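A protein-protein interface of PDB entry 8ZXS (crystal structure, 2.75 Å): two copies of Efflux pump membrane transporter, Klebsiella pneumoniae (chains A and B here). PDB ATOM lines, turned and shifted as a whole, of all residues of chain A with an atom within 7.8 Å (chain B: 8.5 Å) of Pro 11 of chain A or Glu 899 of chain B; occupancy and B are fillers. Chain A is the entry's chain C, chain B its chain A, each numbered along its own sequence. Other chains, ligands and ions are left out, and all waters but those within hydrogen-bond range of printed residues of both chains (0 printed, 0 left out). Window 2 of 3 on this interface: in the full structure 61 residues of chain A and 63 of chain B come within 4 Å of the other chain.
Of chain B, only Glu 899 (3.1 Å) comes within 4 Å of Pro 11 of chain A.
Ile 12 of chain A touches just these residues of chain B: Ala 895 (3.4 Å), Glu 899 (2.7 Å), Ser 900 (3.6 Å) and Trp 901 (3.4 Å).
Of the printed residues of chain A, Ala 895 of chain B touches Ile 12 (3.4 Å) and Val 16 (3.7 Å).
Of the printed residues of chain B, Arg 10 of chain A touches Ala 896 (3.2 Å), Leu 897 (3.5 Å) and Glu 899 (3.0 Å).
The nearest residue of chain B that does not touch Pro 11 of chain A is Trp 901 of chain B (6.1 Å).
The nearest printed residue of chain A that does not touch Leu 897 of chain B is Phe 13 of chain A (5.2 Å).
N of Pro 11 of chain A lies close to OE2 of Glu 899 of chain B, at 3.1 Å.
The backbone NH (N) of Ile 12 of chain A sits at hydrogen-bond distance from the side-chain carboxylate (OE2) of Glu 899 of chain B (2.7 Å).
The backbone carbonyl oxygen (O) of Ala 896 of chain B sits at hydrogen-bond distance from the guanidinium group (NH2) of Arg 10 of chain A, 3.2 Å away.
The backbone carbonyl oxygen (O) of Leu 897 of chain B is in hydrogen-bond range of the guanidinium group (NH2) of Arg 10 of chain A, 3.5 Å away.
The side-chain carboxylate (OE1) of Glu 899 of chain B lies within salt-bridge range of the guanidinium group (NE) of Arg 10 of chain A (3.3 Å).
Ile 12 of chain A touches Ala 895 of chain B (CG2 to O, 3.4 Å).
Ser 900 of chain B touches Ile 12 of chain A.
Trp 901 of chain B touches Ile 12 of chain A (CD1 to CD1, 3.4 Å).
O of Ala 896 of chain B touches CD2 of Phe 13 of chain A, at 3.6 Å.
Phe 13 of chain A touches Glu 899 of chain B (N to OE1, 3.7 Å).
CB of Ala 15 of chain A touches CZ2 of Trp 901 of chain B, 3.7 Å away.
CG2 of Val 16 of chain A touches O of Leu 892 of chain B, at 3.4 Å.
Ala 895 of chain B touches Val 16 of chain A (CB to CG2, 3.7 Å).
Ala 896 of chain B touches Val 16 of chain A.
No position is printed for both chains.
Of the 14 pairs that touch across the chains among the printed residues, none has its exchanged pair printed and touching as well.
N of Ser 900 of chain B lies within hydrogen-bond range of O of Ala 895 of chain B (3.4 Å).
The backbone NH of Leu 903 of chain B sits at hydrogen-bond distance from the side-chain hydroxyl of Ser 900 of chain B (2.6 Å).
N of Thr 902 of chain B sits at hydrogen-bond distance from OG of Ser 900 of chain B, at 2.8 Å.
Of the 17 printed residues of chain B, 7 touch a printed residue of chain A.
Printed residues of chain B that touch a printed residue of chain A: Leu 892, Ala 895, Ala 896, Leu 897, Glu 899, Ser 900 and Trp 901.
Hydrophobic or aromatic side chains of chain B that line the printed part of chain A: Leu 892, Ala 895, Ala 896 and Trp 901.
Printed residues of chain A that touch a printed residue of chain B: Arg 10, Pro 11, Ile 12, Phe 13, Ala 15 and Val 16.
Hydrophobic or aromatic side chains of chain A within 4 Å of the printed part of chain B: Pro 11, Ile 12, Phe 13, Ala 15 and Val 16.
Along chain A the printed residues that touch a printed residue of chain B span positions 10 to 16.
Among the printed residues, Asp or Glu carboxylates within 4 Å of a Lys or Arg side-chain nitrogen of the other chain: Arg 10 of chain A with Glu 899 of chain B.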
ATOM      1  N   PHE A   6      30.502 -37.184   3.412  1.00  0.00           N
ATOM      2  CA  PHE A   6      30.328 -36.983   1.979  1.00  0.00           C
ATOM      3  C   PHE A   6      29.542 -35.711   1.702  1.00  0.00           C
ATOM      4  O   PHE A   6      29.852 -34.970   0.762  1.00  0.00           O
ATOM      5  CB  PHE A   6      29.622 -38.193   1.358  1.00  0.00           C
ATOM      6  CG  PHE A   6      29.117 -37.957  -0.045  1.00  0.00           C
ATOM      7  CD1 PHE A   6      29.912 -38.256  -1.137  1.00  0.00           C
ATOM      8  CD2 PHE A   6      27.843 -37.452  -0.271  1.00  0.00           C
ATOM      9  CE1 PHE A   6      29.455 -38.047  -2.425  1.00  0.00           C
ATOM     10  CE2 PHE A   6      27.384 -37.235  -1.556  1.00  0.00           C
ATOM     11  CZ  PHE A   6      28.191 -37.536  -2.633  1.00  0.00           C
ATOM     12  N   PHE A   7      28.506 -35.450   2.498  1.00  0.00           N
ATOM     13  CA  PHE A   7      27.644 -34.327   2.142  1.00  0.00           C
ATOM     14  C   PHE A   7      28.257 -32.966   2.484  1.00  0.00           C
ATOM     15  O   PHE A   7      28.081 -32.009   1.721  1.00  0.00           O
ATOM     16  CB  PHE A   7      26.271 -34.497   2.785  1.00  0.00           C
ATOM     17  CG  PHE A   7      25.304 -35.235   1.908  1.00  0.00           C
ATOM     18  CD1 PHE A   7      24.693 -34.595   0.847  1.00  0.00           C
ATOM     19  CD2 PHE A   7      25.040 -36.576   2.119  1.00  0.00           C
ATOM     20  CE1 PHE A   7      23.819 -35.268   0.028  1.00  0.00           C
ATOM     21  CE2 PHE A   7      24.168 -37.253   1.305  1.00  0.00           C
ATOM     22  CZ  PHE A   7      23.555 -36.601   0.257  1.00  0.00           C
ATOM     23  N   ILE A   8      28.982 -32.845   3.603  1.00  0.00           N
ATOM     24  CA  ILE A   8      29.527 -31.534   3.968  1.00  0.00           C
ATOM     25  C   ILE A   8      30.624 -31.113   3.003  1.00  0.00           C
ATOM     26  O   ILE A   8      30.839 -29.914   2.783  1.00  0.00           O
ATOM     27  CB  ILE A   8      30.044 -31.502   5.420  1.00  0.00           C
ATOM     28  CG1 ILE A   8      30.874 -32.741   5.755  1.00  0.00           C
ATOM     29  CG2 ILE A   8      28.903 -31.357   6.385  1.00  0.00           C
ATOM     30  CD1 ILE A   8      31.167 -32.877   7.241  1.00  0.00           C
ATOM     31  N   ASP A   9      31.346 -32.071   2.428  1.00  0.00           N
ATOM     32  CA  ASP A   9      32.352 -31.736   1.434  1.00  0.00           C
ATOM     33  C   ASP A   9      31.752 -31.495   0.058  1.00  0.00           C
ATOM     34  O   ASP A   9      32.477 -31.076  -0.851  1.00  0.00           O
ATOM     35  CB  ASP A   9      33.411 -32.842   1.362  1.00  0.00           C
ATOM     36  CG  ASP A   9      34.216 -32.961   2.649  1.00  0.00           C
ATOM     37  OD1 ASP A   9      34.307 -31.958   3.393  1.00  0.00           O
ATOM     38  OD2 ASP A   9      34.753 -34.056   2.919  1.00  0.00           O
ATOM     39  N   ARG A  10      30.455 -31.749  -0.116  1.00  0.00           N
ATOM     40  CA  ARG A  10      29.747 -31.503  -1.374  1.00  0.00           C
ATOM     41  C   ARG A  10      28.457 -30.743  -1.075  1.00  0.00           C
ATOM     42  O   ARG A  10      27.355 -31.264  -1.271  1.00  0.00           O
ATOM     43  CB  ARG A  10      29.458 -32.817  -2.102  1.00  0.00           C
ATOM     44  CG  ARG A  10      30.644 -33.781  -2.175  1.00  0.00           C
ATOM     45  CD  ARG A  10      30.493 -34.777  -3.318  1.00  0.00           C
ATOM     46  NE  ARG A  10      30.171 -34.116  -4.578  1.00  0.00           N
ATOM     47  CZ  ARG A  10      30.420 -34.621  -5.780  1.00  0.00           C
ATOM     48  NH1 ARG A  10      31.005 -35.800  -5.928  1.00  0.00           N
ATOM     49  NH2 ARG A  10      30.074 -33.927  -6.860  1.00  0.00           N
ATOM     50  N   PRO A  11      28.563 -29.496  -0.603  1.00  0.00           N
ATOM     51  CA  PRO A  11      27.352 -28.768  -0.178  1.00  0.00           C
ATOM     52  C   PRO A  11      26.336 -28.542  -1.288  1.00  0.00           C
ATOM     53  O   PRO A  11      25.128 -28.493  -1.010  1.00  0.00           O
ATOM     54  CB  PRO A  11      27.911 -27.439   0.354  1.00  0.00           C
ATOM     55  CG  PRO A  11      29.234 -27.288  -0.314  1.00  0.00           C
ATOM     56  CD  PRO A  11      29.779 -28.673  -0.459  1.00  0.00           C
ATOM     57  N   ILE A  12      26.781 -28.394  -2.538  1.00  0.00           N
ATOM     58  CA  ILE A  12      25.825 -28.194  -3.622  1.00  0.00           C
ATOM     59  C   ILE A  12      24.955 -29.431  -3.795  1.00  0.00           C
ATOM     60  O   ILE A  12      23.761 -29.322  -4.095  1.00  0.00           O
ATOM     61  CB  ILE A  12      26.564 -27.814  -4.920  1.00  0.00           C
ATOM     62  CG1 ILE A  12      27.217 -26.439  -4.754  1.00  0.00           C
ATOM     63  CG2 ILE A  12      25.609 -27.851  -6.117  1.00  0.00           C
ATOM     64  CD1 ILE A  12      27.446 -25.696  -6.042  1.00  0.00           C
ATOM     65  N   PHE A  13      25.526 -30.619  -3.583  1.00  0.00           N
ATOM     66  CA  PHE A  13      24.739 -31.848  -3.593  1.00  0.00           C
ATOM     67  C   PHE A  13      23.633 -31.805  -2.544  1.00  0.00           C
ATOM     68  O   PHE A  13      22.485 -32.186  -2.817  1.00  0.00           O
ATOM     69  CB  PHE A  13      25.667 -33.040  -3.351  1.00  0.00           C
ATOM     70  CG  PHE A  13      25.179 -34.330  -3.940  1.00  0.00           C
ATOM     71  CD1 PHE A  13      24.029 -34.938  -3.463  1.00  0.00           C
ATOM     72  CD2 PHE A  13      25.880 -34.947  -4.961  1.00  0.00           C
ATOM     73  CE1 PHE A  13      23.582 -36.129  -4.001  1.00  0.00           C
ATOM     74  CE2 PHE A  13      25.437 -36.140  -5.503  1.00  0.00           C
ATOM     75  CZ  PHE A  13      24.288 -36.731  -5.020  1.00  0.00           C
ATOM     76  N   ALA A  14      23.963 -31.350  -1.332  1.00  0.00           N
ATOM     77  CA  ALA A  14      22.969 -31.266  -0.266  1.00  0.00           C
ATOM     78  C   ALA A  14      21.861 -30.279  -0.619  1.00  0.00           C
ATOM     79  O   ALA A  14      20.668 -30.554  -0.397  1.00  0.00           O
ATOM     80  CB  ALA A  14      23.656 -30.867   1.039  1.00  0.00           C
ATOM     81  N   ALA A  15      22.241 -29.123  -1.169  1.00  0.00           N
ATOM     82  CA  ALA A  15      21.242 -28.158  -1.613  1.00  0.00           C
ATOM     83  C   ALA A  15      20.347 -28.762  -2.689  1.00  0.00           C
ATOM     84  O   ALA A  15      19.127 -28.573  -2.670  1.00  0.00           O
ATOM     85  CB  ALA A  15      21.922 -26.890  -2.129  1.00  0.00           C
ATOM     86  N   VAL A  16      20.941 -29.506  -3.623  1.00  0.00           N
ATOM     87  CA  VAL A  16      20.178 -30.109  -4.710  1.00  0.00           C
ATOM     88  C   VAL A  16      19.166 -31.108  -4.163  1.00  0.00           C
ATOM     89  O   VAL A  16      18.017 -31.160  -4.615  1.00  0.00           O
ATOM     90  CB  VAL A  16      21.135 -30.764  -5.723  1.00  0.00           C
ATOM     91  CG1 VAL A  16      20.422 -31.858  -6.505  1.00  0.00           C
ATOM     92  CG2 VAL A  16      21.720 -29.714  -6.655  1.00  0.00           C
ATOM     93  N   LEU A  17      19.576 -31.920  -3.187  1.00  0.00           N
ATOM     94  CA  LEU A  17      18.660 -32.906  -2.617  1.00  0.00           C
ATOM     95  C   LEU A  17      17.476 -32.228  -1.931  1.00  0.00           C
ATOM     96  O   LEU A  17      16.306 -32.584  -2.168  1.00  0.00           O
ATOM     97  CB  LEU A  17      19.407 -33.804  -1.636  1.00  0.00           C
ATOM     98  CG  LEU A  17      18.998 -35.274  -1.597  1.00  0.00           C
ATOM     99  CD1 LEU A  17      19.519 -35.989  -2.835  1.00  0.00           C
ATOM    100  CD2 LEU A  17      19.512 -35.935  -0.322  1.00  0.00           C
ATOM    101  N   THR A 489      22.251 -33.861   5.961  1.00  0.00           N
ATOM    102  CA  THR A 489      22.902 -33.564   4.689  1.00  0.00           C
ATOM    103  C   THR A 489      23.213 -32.082   4.512  1.00  0.00           C
ATOM    104  O   THR A 489      24.375 -31.719   4.316  1.00  0.00           O
ATOM    105  CB  THR A 489      22.045 -34.080   3.512  1.00  0.00           C
ATOM    106  OG1 THR A 489      20.750 -33.465   3.531  1.00  0.00           O
ATOM    107  CG2 THR A 489      21.888 -35.597   3.577  1.00  0.00           C
ATOM    108  N   LEU A 490      22.211 -31.206   4.580  1.00  0.00           N
ATOM    109  CA  LEU A 490      22.414 -29.807   4.225  1.00  0.00           C
ATOM    110  C   LEU A 490      22.722 -28.928   5.428  1.00  0.00           C
ATOM    111  O   LEU A 490      23.450 -27.937   5.290  1.00  0.00           O
ATOM    112  CB  LEU A 490      21.178 -29.274   3.492  1.00  0.00           C
ATOM    113  CG  LEU A 490      21.042 -27.765   3.271  1.00  0.00           C
ATOM    114  CD1 LEU A 490      21.927 -27.315   2.132  1.00  0.00           C
ATOM    115  CD2 LEU A 490      19.611 -27.396   2.993  1.00  0.00           C
ATOM    116  N   PRO A 492      24.687 -29.400   8.254  1.00  0.00           N
ATOM    117  CA  PRO A 492      26.113 -29.216   8.558  1.00  0.00           C
ATOM    118  C   PRO A 492      26.882 -28.523   7.448  1.00  0.00           C
ATOM    119  O   PRO A 492      27.844 -27.803   7.739  1.00  0.00           O
ATOM    120  CB  PRO A 492      26.612 -30.647   8.780  1.00  0.00           C
ATOM    121  CG  PRO A 492      25.696 -31.488   7.961  1.00  0.00           C
ATOM    122  CD  PRO A 492      24.358 -30.823   8.037  1.00  0.00           C
ATOM    123  N   ALA A 493      26.496 -28.721   6.186  1.00  0.00           N
ATOM    124  CA  ALA A 493      27.177 -28.037   5.093  1.00  0.00           C
ATOM    125  C   ALA A 493      26.988 -26.530   5.198  1.00  0.00           C
ATOM    126  O   ALA A 493      27.960 -25.766   5.179  1.00  0.00           O
ATOM    127  CB  ALA A 493      26.667 -28.562   3.750  1.00  0.00           C
ATOM    128  N   LEU A 494      25.733 -26.087   5.327  1.00  0.00           N
ATOM    129  CA  LEU A 494      25.462 -24.666   5.510  1.00  0.00           C
ATOM    130  C   LEU A 494      26.106 -24.137   6.783  1.00  0.00           C
ATOM    131  O   LEU A 494      26.515 -22.973   6.830  1.00  0.00           O
ATOM    132  CB  LEU A 494      23.956 -24.422   5.532  1.00  0.00           C
ATOM    133  CG  LEU A 494      23.227 -24.466   4.187  1.00  0.00           C
ATOM    134  CD1 LEU A 494      21.996 -23.567   4.190  1.00  0.00           C
ATOM    135  CD2 LEU A 494      24.168 -24.090   3.048  1.00  0.00           C
ATOM    136  N   ALA A 496      29.037 -25.215   8.047  1.00  0.00           N
ATOM    137  CA  ALA A 496      30.458 -25.055   7.752  1.00  0.00           C
ATOM    138  C   ALA A 496      30.702 -23.834   6.879  1.00  0.00           C
ATOM    139  O   ALA A 496      31.701 -23.126   7.053  1.00  0.00           O
ATOM    140  CB  ALA A 496      31.008 -26.311   7.078  1.00  0.00           C
ATOM    141  N   LEU A 497      29.806 -23.574   5.935  1.00  0.00           N
ATOM    142  CA  LEU A 497      29.993 -22.467   5.008  1.00  0.00           C
ATOM    143  C   LEU A 497      29.491 -21.128   5.540  1.00  0.00           C
ATOM    144  O   LEU A 497      29.878 -20.086   5.000  1.00  0.00           O
ATOM    145  CB  LEU A 497      29.307 -22.782   3.674  1.00  0.00           C
ATOM    146  CG  LEU A 497      30.093 -23.686   2.723  1.00  0.00           C
ATOM    147  CD1 LEU A 497      29.785 -25.166   2.901  1.00  0.00           C
ATOM    148  CD2 LEU A 497      29.794 -23.268   1.315  1.00  0.00           C
ATOM    149  N   PHE B 891      18.801 -29.738 -14.548  1.00  0.00           N
ATOM    150  CA  PHE B 891      19.754 -28.801 -13.972  1.00  0.00           C
ATOM    151  C   PHE B 891      20.176 -29.278 -12.593  1.00  0.00           C
ATOM    152  O   PHE B 891      21.371 -29.443 -12.318  1.00  0.00           O
ATOM    153  CB  PHE B 891      19.129 -27.404 -13.909  1.00  0.00           C
ATOM    154  CG  PHE B 891      19.928 -26.408 -13.111  1.00  0.00           C
ATOM    155  CD1 PHE B 891      20.923 -25.654 -13.714  1.00  0.00           C
ATOM    156  CD2 PHE B 891      19.671 -26.212 -11.761  1.00  0.00           C
ATOM    157  CE1 PHE B 891      21.654 -24.737 -12.985  1.00  0.00           C
ATOM    158  CE2 PHE B 891      20.400 -25.297 -11.028  1.00  0.00           C
ATOM    159  CZ  PHE B 891      21.392 -24.558 -11.641  1.00  0.00           C
ATOM    160  N   LEU B 892      19.192 -29.605 -11.750  1.00  0.00           N
ATOM    161  CA  LEU B 892      19.504 -30.003 -10.386  1.00  0.00           C
ATOM    162  C   LEU B 892      20.447 -31.195 -10.385  1.00  0.00           C
ATOM    163  O   LEU B 892      21.502 -31.167  -9.736  1.00  0.00           O
ATOM    164  CB  LEU B 892      18.215 -30.307  -9.628  1.00  0.00           C
ATOM    165  CG  LEU B 892      17.557 -29.043  -9.072  1.00  0.00           C
ATOM    166  CD1 LEU B 892      16.173 -29.342  -8.510  1.00  0.00           C
ATOM    167  CD2 LEU B 892      18.455 -28.394  -8.018  1.00  0.00           C
ATOM    168  N   VAL B 893      20.134 -32.213 -11.190  1.00  0.00           N
ATOM    169  CA  VAL B 893      20.988 -33.395 -11.234  1.00  0.00           C
ATOM    170  C   VAL B 893      22.394 -32.996 -11.650  1.00  0.00           C
ATOM    171  O   VAL B 893      23.383 -33.357 -10.997  1.00  0.00           O
ATOM    172  CB  VAL B 893      20.398 -34.455 -12.179  1.00  0.00           C
ATOM    173  CG1 VAL B 893      21.254 -35.712 -12.162  1.00  0.00           C
ATOM    174  CG2 VAL B 893      18.958 -34.770 -11.802  1.00  0.00           C
ATOM    175  N   LEU B 894      22.497 -32.182 -12.703  1.00  0.00           N
ATOM    176  CA  LEU B 894      23.811 -31.764 -13.173  1.00  0.00           C
ATOM    177  C   LEU B 894      24.526 -30.955 -12.103  1.00  0.00           C
ATOM    178  O   LEU B 894      25.731 -31.134 -11.880  1.00  0.00           O
ATOM    179  CB  LEU B 894      23.675 -30.972 -14.473  1.00  0.00           C
ATOM    180  CG  LEU B 894      23.422 -31.846 -15.703  1.00  0.00           C
ATOM    181  CD1 LEU B 894      23.185 -31.000 -16.945  1.00  0.00           C
ATOM    182  CD2 LEU B 894      24.582 -32.809 -15.912  1.00  0.00           C
ATOM    183  N   ALA B 895      23.784 -30.098 -11.391  1.00  0.00           N
ATOM    184  CA  ALA B 895      24.398 -29.326 -10.319  1.00  0.00           C
ATOM    185  C   ALA B 895      25.026 -30.247  -9.287  1.00  0.00           C
ATOM    186  O   ALA B 895      26.105 -29.955  -8.759  1.00  0.00           O
ATOM    187  CB  ALA B 895      23.363 -28.408  -9.668  1.00  0.00           C
ATOM    188  N   ALA B 896      24.376 -31.380  -9.008  1.00  0.00           N
ATOM    189  CA  ALA B 896      24.945 -32.327  -8.057  1.00  0.00           C
ATOM    190  C   ALA B 896      26.190 -32.995  -8.627  1.00  0.00           C
ATOM    191  O   ALA B 896      27.165 -33.223  -7.901  1.00  0.00           O
ATOM    192  CB  ALA B 896      23.902 -33.370  -7.662  1.00  0.00           C
ATOM    193  N   LEU B 897      26.183 -33.309  -9.925  1.00  0.00           N
ATOM    194  CA  LEU B 897      27.314 -34.034 -10.494  1.00  0.00           C
ATOM    195  C   LEU B 897      28.547 -33.146 -10.594  1.00  0.00           C
ATOM    196  O   LEU B 897      29.662 -33.585 -10.285  1.00  0.00           O
ATOM    197  CB  LEU B 897      26.942 -34.607 -11.863  1.00  0.00           C
ATOM    198  CG  LEU B 897      28.094 -35.234 -12.653  1.00  0.00           C
ATOM    199  CD1 LEU B 897      28.254 -36.704 -12.306  1.00  0.00           C
ATOM    200  CD2 LEU B 897      27.864 -35.065 -14.146  1.00  0.00           C
ATOM    201  N   TYR B 898      28.366 -31.897 -11.016  1.00  0.00           N
ATOM    202  CA  TYR B 898      29.474 -30.971 -11.209  1.00  0.00           C
ATOM    203  C   TYR B 898      29.881 -30.235  -9.940  1.00  0.00           C
ATOM    204  O   TYR B 898      30.959 -29.631  -9.920  1.00  0.00           O
ATOM    205  CB  TYR B 898      29.115 -29.938 -12.280  1.00  0.00           C
ATOM    206  CG  TYR B 898      28.880 -30.518 -13.652  1.00  0.00           C
ATOM    207  CD1 TYR B 898      29.558 -31.653 -14.077  1.00  0.00           C
ATOM    208  CD2 TYR B 898      27.978 -29.925 -14.524  1.00  0.00           C
ATOM    209  CE1 TYR B 898      29.344 -32.181 -15.337  1.00  0.00           C
ATOM    210  CE2 TYR B 898      27.755 -30.446 -15.782  1.00  0.00           C
ATOM    211  CZ  TYR B 898      28.436 -31.574 -16.181  1.00  0.00           C
ATOM    212  OH  TYR B 898      28.213 -32.083 -17.434  1.00  0.00           O
ATOM    213  N   GLU B 899      29.059 -30.275  -8.890  1.00  0.00           N
ATOM    214  CA  GLU B 899      29.271 -29.448  -7.702  1.00  0.00           C
ATOM    215  C   GLU B 899      29.341 -27.970  -8.079  1.00  0.00           C
ATOM    216  O   GLU B 899      30.187 -27.220  -7.590  1.00  0.00           O
ATOM    217  CB  GLU B 899      30.527 -29.884  -6.938  1.00  0.00           C
ATOM    218  CG  GLU B 899      30.566 -29.484  -5.464  1.00  0.00           C
ATOM    219  CD  GLU B 899      29.391 -30.024  -4.667  1.00  0.00           C
ATOM    220  OE1 GLU B 899      28.862 -31.105  -5.021  1.00  0.00           O
ATOM    221  OE2 GLU B 899      29.003 -29.369  -3.677  1.00  0.00           O
ATOM    222  N   SER B 900      28.445 -27.546  -8.971  1.00  0.00           N
ATOM    223  CA  SER B 900      28.440 -26.176  -9.459  1.00  0.00           C
ATOM    224  C   SER B 900      27.027 -25.772  -9.853  1.00  0.00           C
ATOM    225  O   SER B 900      26.290 -26.567 -10.442  1.00  0.00           O
ATOM    226  CB  SER B 900      29.385 -26.015 -10.655  1.00  0.00           C
ATOM    227  OG  SER B 900      28.866 -25.083 -11.589  1.00  0.00           O
ATOM    228  N   TRP B 901      26.660 -24.528  -9.534  1.00  0.00           N
ATOM    229  CA  TRP B 901      25.393 -23.955  -9.974  1.00  0.00           C
ATOM    230  C   TRP B 901      25.454 -23.399 -11.392  1.00  0.00           C
ATOM    231  O   TRP B 901      24.421 -22.965 -11.912  1.00  0.00           O
ATOM    232  CB  TRP B 901      24.951 -22.824  -9.037  1.00  0.00           C
ATOM    233  CG  TRP B 901      24.654 -23.228  -7.625  1.00  0.00           C
ATOM    234  CD1 TRP B 901      25.451 -23.037  -6.538  1.00  0.00           C
ATOM    235  CD2 TRP B 901      23.461 -23.862  -7.143  1.00  0.00           C
ATOM    236  NE1 TRP B 901      24.839 -23.526  -5.411  1.00  0.00           N
ATOM    237  CE2 TRP B 901      23.616 -24.036  -5.754  1.00  0.00           C
ATOM    238  CE3 TRP B 901      22.284 -24.304  -7.752  1.00  0.00           C
ATOM    239  CZ2 TRP B 901      22.637 -24.634  -4.964  1.00  0.00           C
ATOM    240  CZ3 TRP B 901      21.314 -24.897  -6.967  1.00  0.00           C
ATOM    241  CH2 TRP B 901      21.497 -25.057  -5.587  1.00  0.00           C
ATOM    242  N   THR B 902      26.627 -23.380 -12.014  1.00  0.00           N
ATOM    243  CA  THR B 902      26.819 -22.753 -13.318  1.00  0.00           C
ATOM    244  C   THR B 902      27.279 -23.726 -14.389  1.00  0.00           C
ATOM    245  O   THR B 902      26.853 -23.609 -15.540  1.00  0.00           O
ATOM    246  CB  THR B 902      27.837 -21.605 -13.211  1.00  0.00           C
ATOM    247  OG1 THR B 902      28.973 -22.042 -12.454  1.00  0.00           O
ATOM    248  CG2 THR B 902      27.217 -20.397 -12.525  1.00  0.00           C
ATOM    249  N   LEU B 903      28.127 -24.688 -14.033  1.00  0.00           N
ATOM    250  CA  LEU B 903      28.586 -25.692 -14.989  1.00  0.00           C
ATOM    251  C   LEU B 903      27.458 -26.409 -15.730  1.00  0.00           C
ATOM    252  O   LEU B 903      27.643 -26.709 -16.923  1.00  0.00           O
ATOM    253  CB  LEU B 903      29.484 -26.705 -14.268  1.00  0.00           C
ATOM    254  CG  LEU B 903      30.989 -26.522 -14.451  1.00  0.00           C
ATOM    255  CD1 LEU B 903      31.410 -27.095 -15.780  1.00  0.00           C
ATOM    256  CD2 LEU B 903      31.382 -25.055 -14.360  1.00  0.00           C
ATOM    257  N   PRO B 904      26.305 -26.725 -15.119  1.00  0.00           N
ATOM    258  CA  PRO B 904      25.202 -27.297 -15.910  1.00  0.00           C
ATOM    259  C   PRO B 904      24.833 -26.485 -17.142  1.00  0.00           C
ATOM    260  O   PRO B 904      24.453 -27.069 -18.165  1.00  0.00           O
ATOM    261  CB  PRO B 904      24.044 -27.336 -14.906  1.00  0.00           C
ATOM    262  CG  PRO B 904      24.699 -27.528 -13.602  1.00  0.00           C
ATOM    263  CD  PRO B 904      26.023 -26.802 -13.672  1.00  0.00           C
ATOM    264  N   GLU B 953      32.282 -32.992 -17.848  1.00  0.00           N
ATOM    265  CA  GLU B 953      32.845 -33.653 -16.675  1.00  0.00           C
ATOM    266  C   GLU B 953      34.302 -34.032 -16.908  1.00  0.00           C
ATOM    267  O   GLU B 953      35.124 -33.942 -15.989  1.00  0.00           O
ATOM    268  CB  GLU B 953      32.021 -34.886 -16.300  1.00  0.00           C
ATOM    269  CG  GLU B 953      31.877 -35.089 -14.791  1.00  0.00           C
ATOM    270  CD  GLU B 953      32.903 -36.055 -14.227  1.00  0.00           C
ATOM    271  OE1 GLU B 953      33.763 -36.533 -14.998  1.00  0.00           O
ATOM    272  OE2 GLU B 953      32.859 -36.328 -13.008  1.00  0.00           O
ATOM    273  N   ARG B 956      36.249 -30.788 -16.417  1.00  0.00           N
ATOM    274  CA  ARG B 956      36.337 -30.404 -15.013  1.00  0.00           C
ATOM    275  C   ARG B 956      37.309 -31.309 -14.262  1.00  0.00           C
ATOM    276  O   ARG B 956      38.145 -30.822 -13.490  1.00  0.00           O
ATOM    277  CB  ARG B 956      34.941 -30.405 -14.379  1.00  0.00           C
ATOM    278  CG  ARG B 956      34.631 -31.541 -13.410  1.00  0.00           C
ATOM    279  CD  ARG B 956      33.522 -31.162 -12.435  1.00  0.00           C
ATOM    280  NE  ARG B 956      33.327 -32.185 -11.417  1.00  0.00           N
ATOM    281  CZ  ARG B 956      33.586 -32.018 -10.127  1.00  0.00           C
ATOM    282  NH1 ARG B 956      34.048 -30.871  -9.658  1.00  0.00           N
ATOM    283  NH2 ARG B 956      33.384 -33.031  -9.289  1.00  0.00           N
ATOM    284  N   ARG B1035      33.406 -20.801 -16.896  1.00  0.00           N
ATOM    285  CA  ARG B1035      34.389 -20.979 -15.839  1.00  0.00           C
ATOM    286  C   ARG B1035      35.314 -19.784 -15.668  1.00  0.00           C
ATOM    287  O   ARG B1035      36.039 -19.730 -14.668  1.00  0.00           O
ATOM    288  CB  ARG B1035      35.214 -22.239 -16.094  1.00  0.00           C
ATOM    289  CG  ARG B1035      34.901 -23.342 -15.110  1.00  0.00           C
ATOM    290  CD  ARG B1035      35.848 -24.506 -15.254  1.00  0.00           C
ATOM    291  NE  ARG B1035      35.812 -25.371 -14.081  1.00  0.00           N
ATOM    292  CZ  ARG B1035      36.355 -25.072 -12.909  1.00  0.00           C
ATOM    293  NH1 ARG B1035      37.022 -23.944 -12.721  1.00  0.00           N
ATOM    294  NH2 ARG B1035      36.232 -25.932 -11.902  1.00  0.00           N
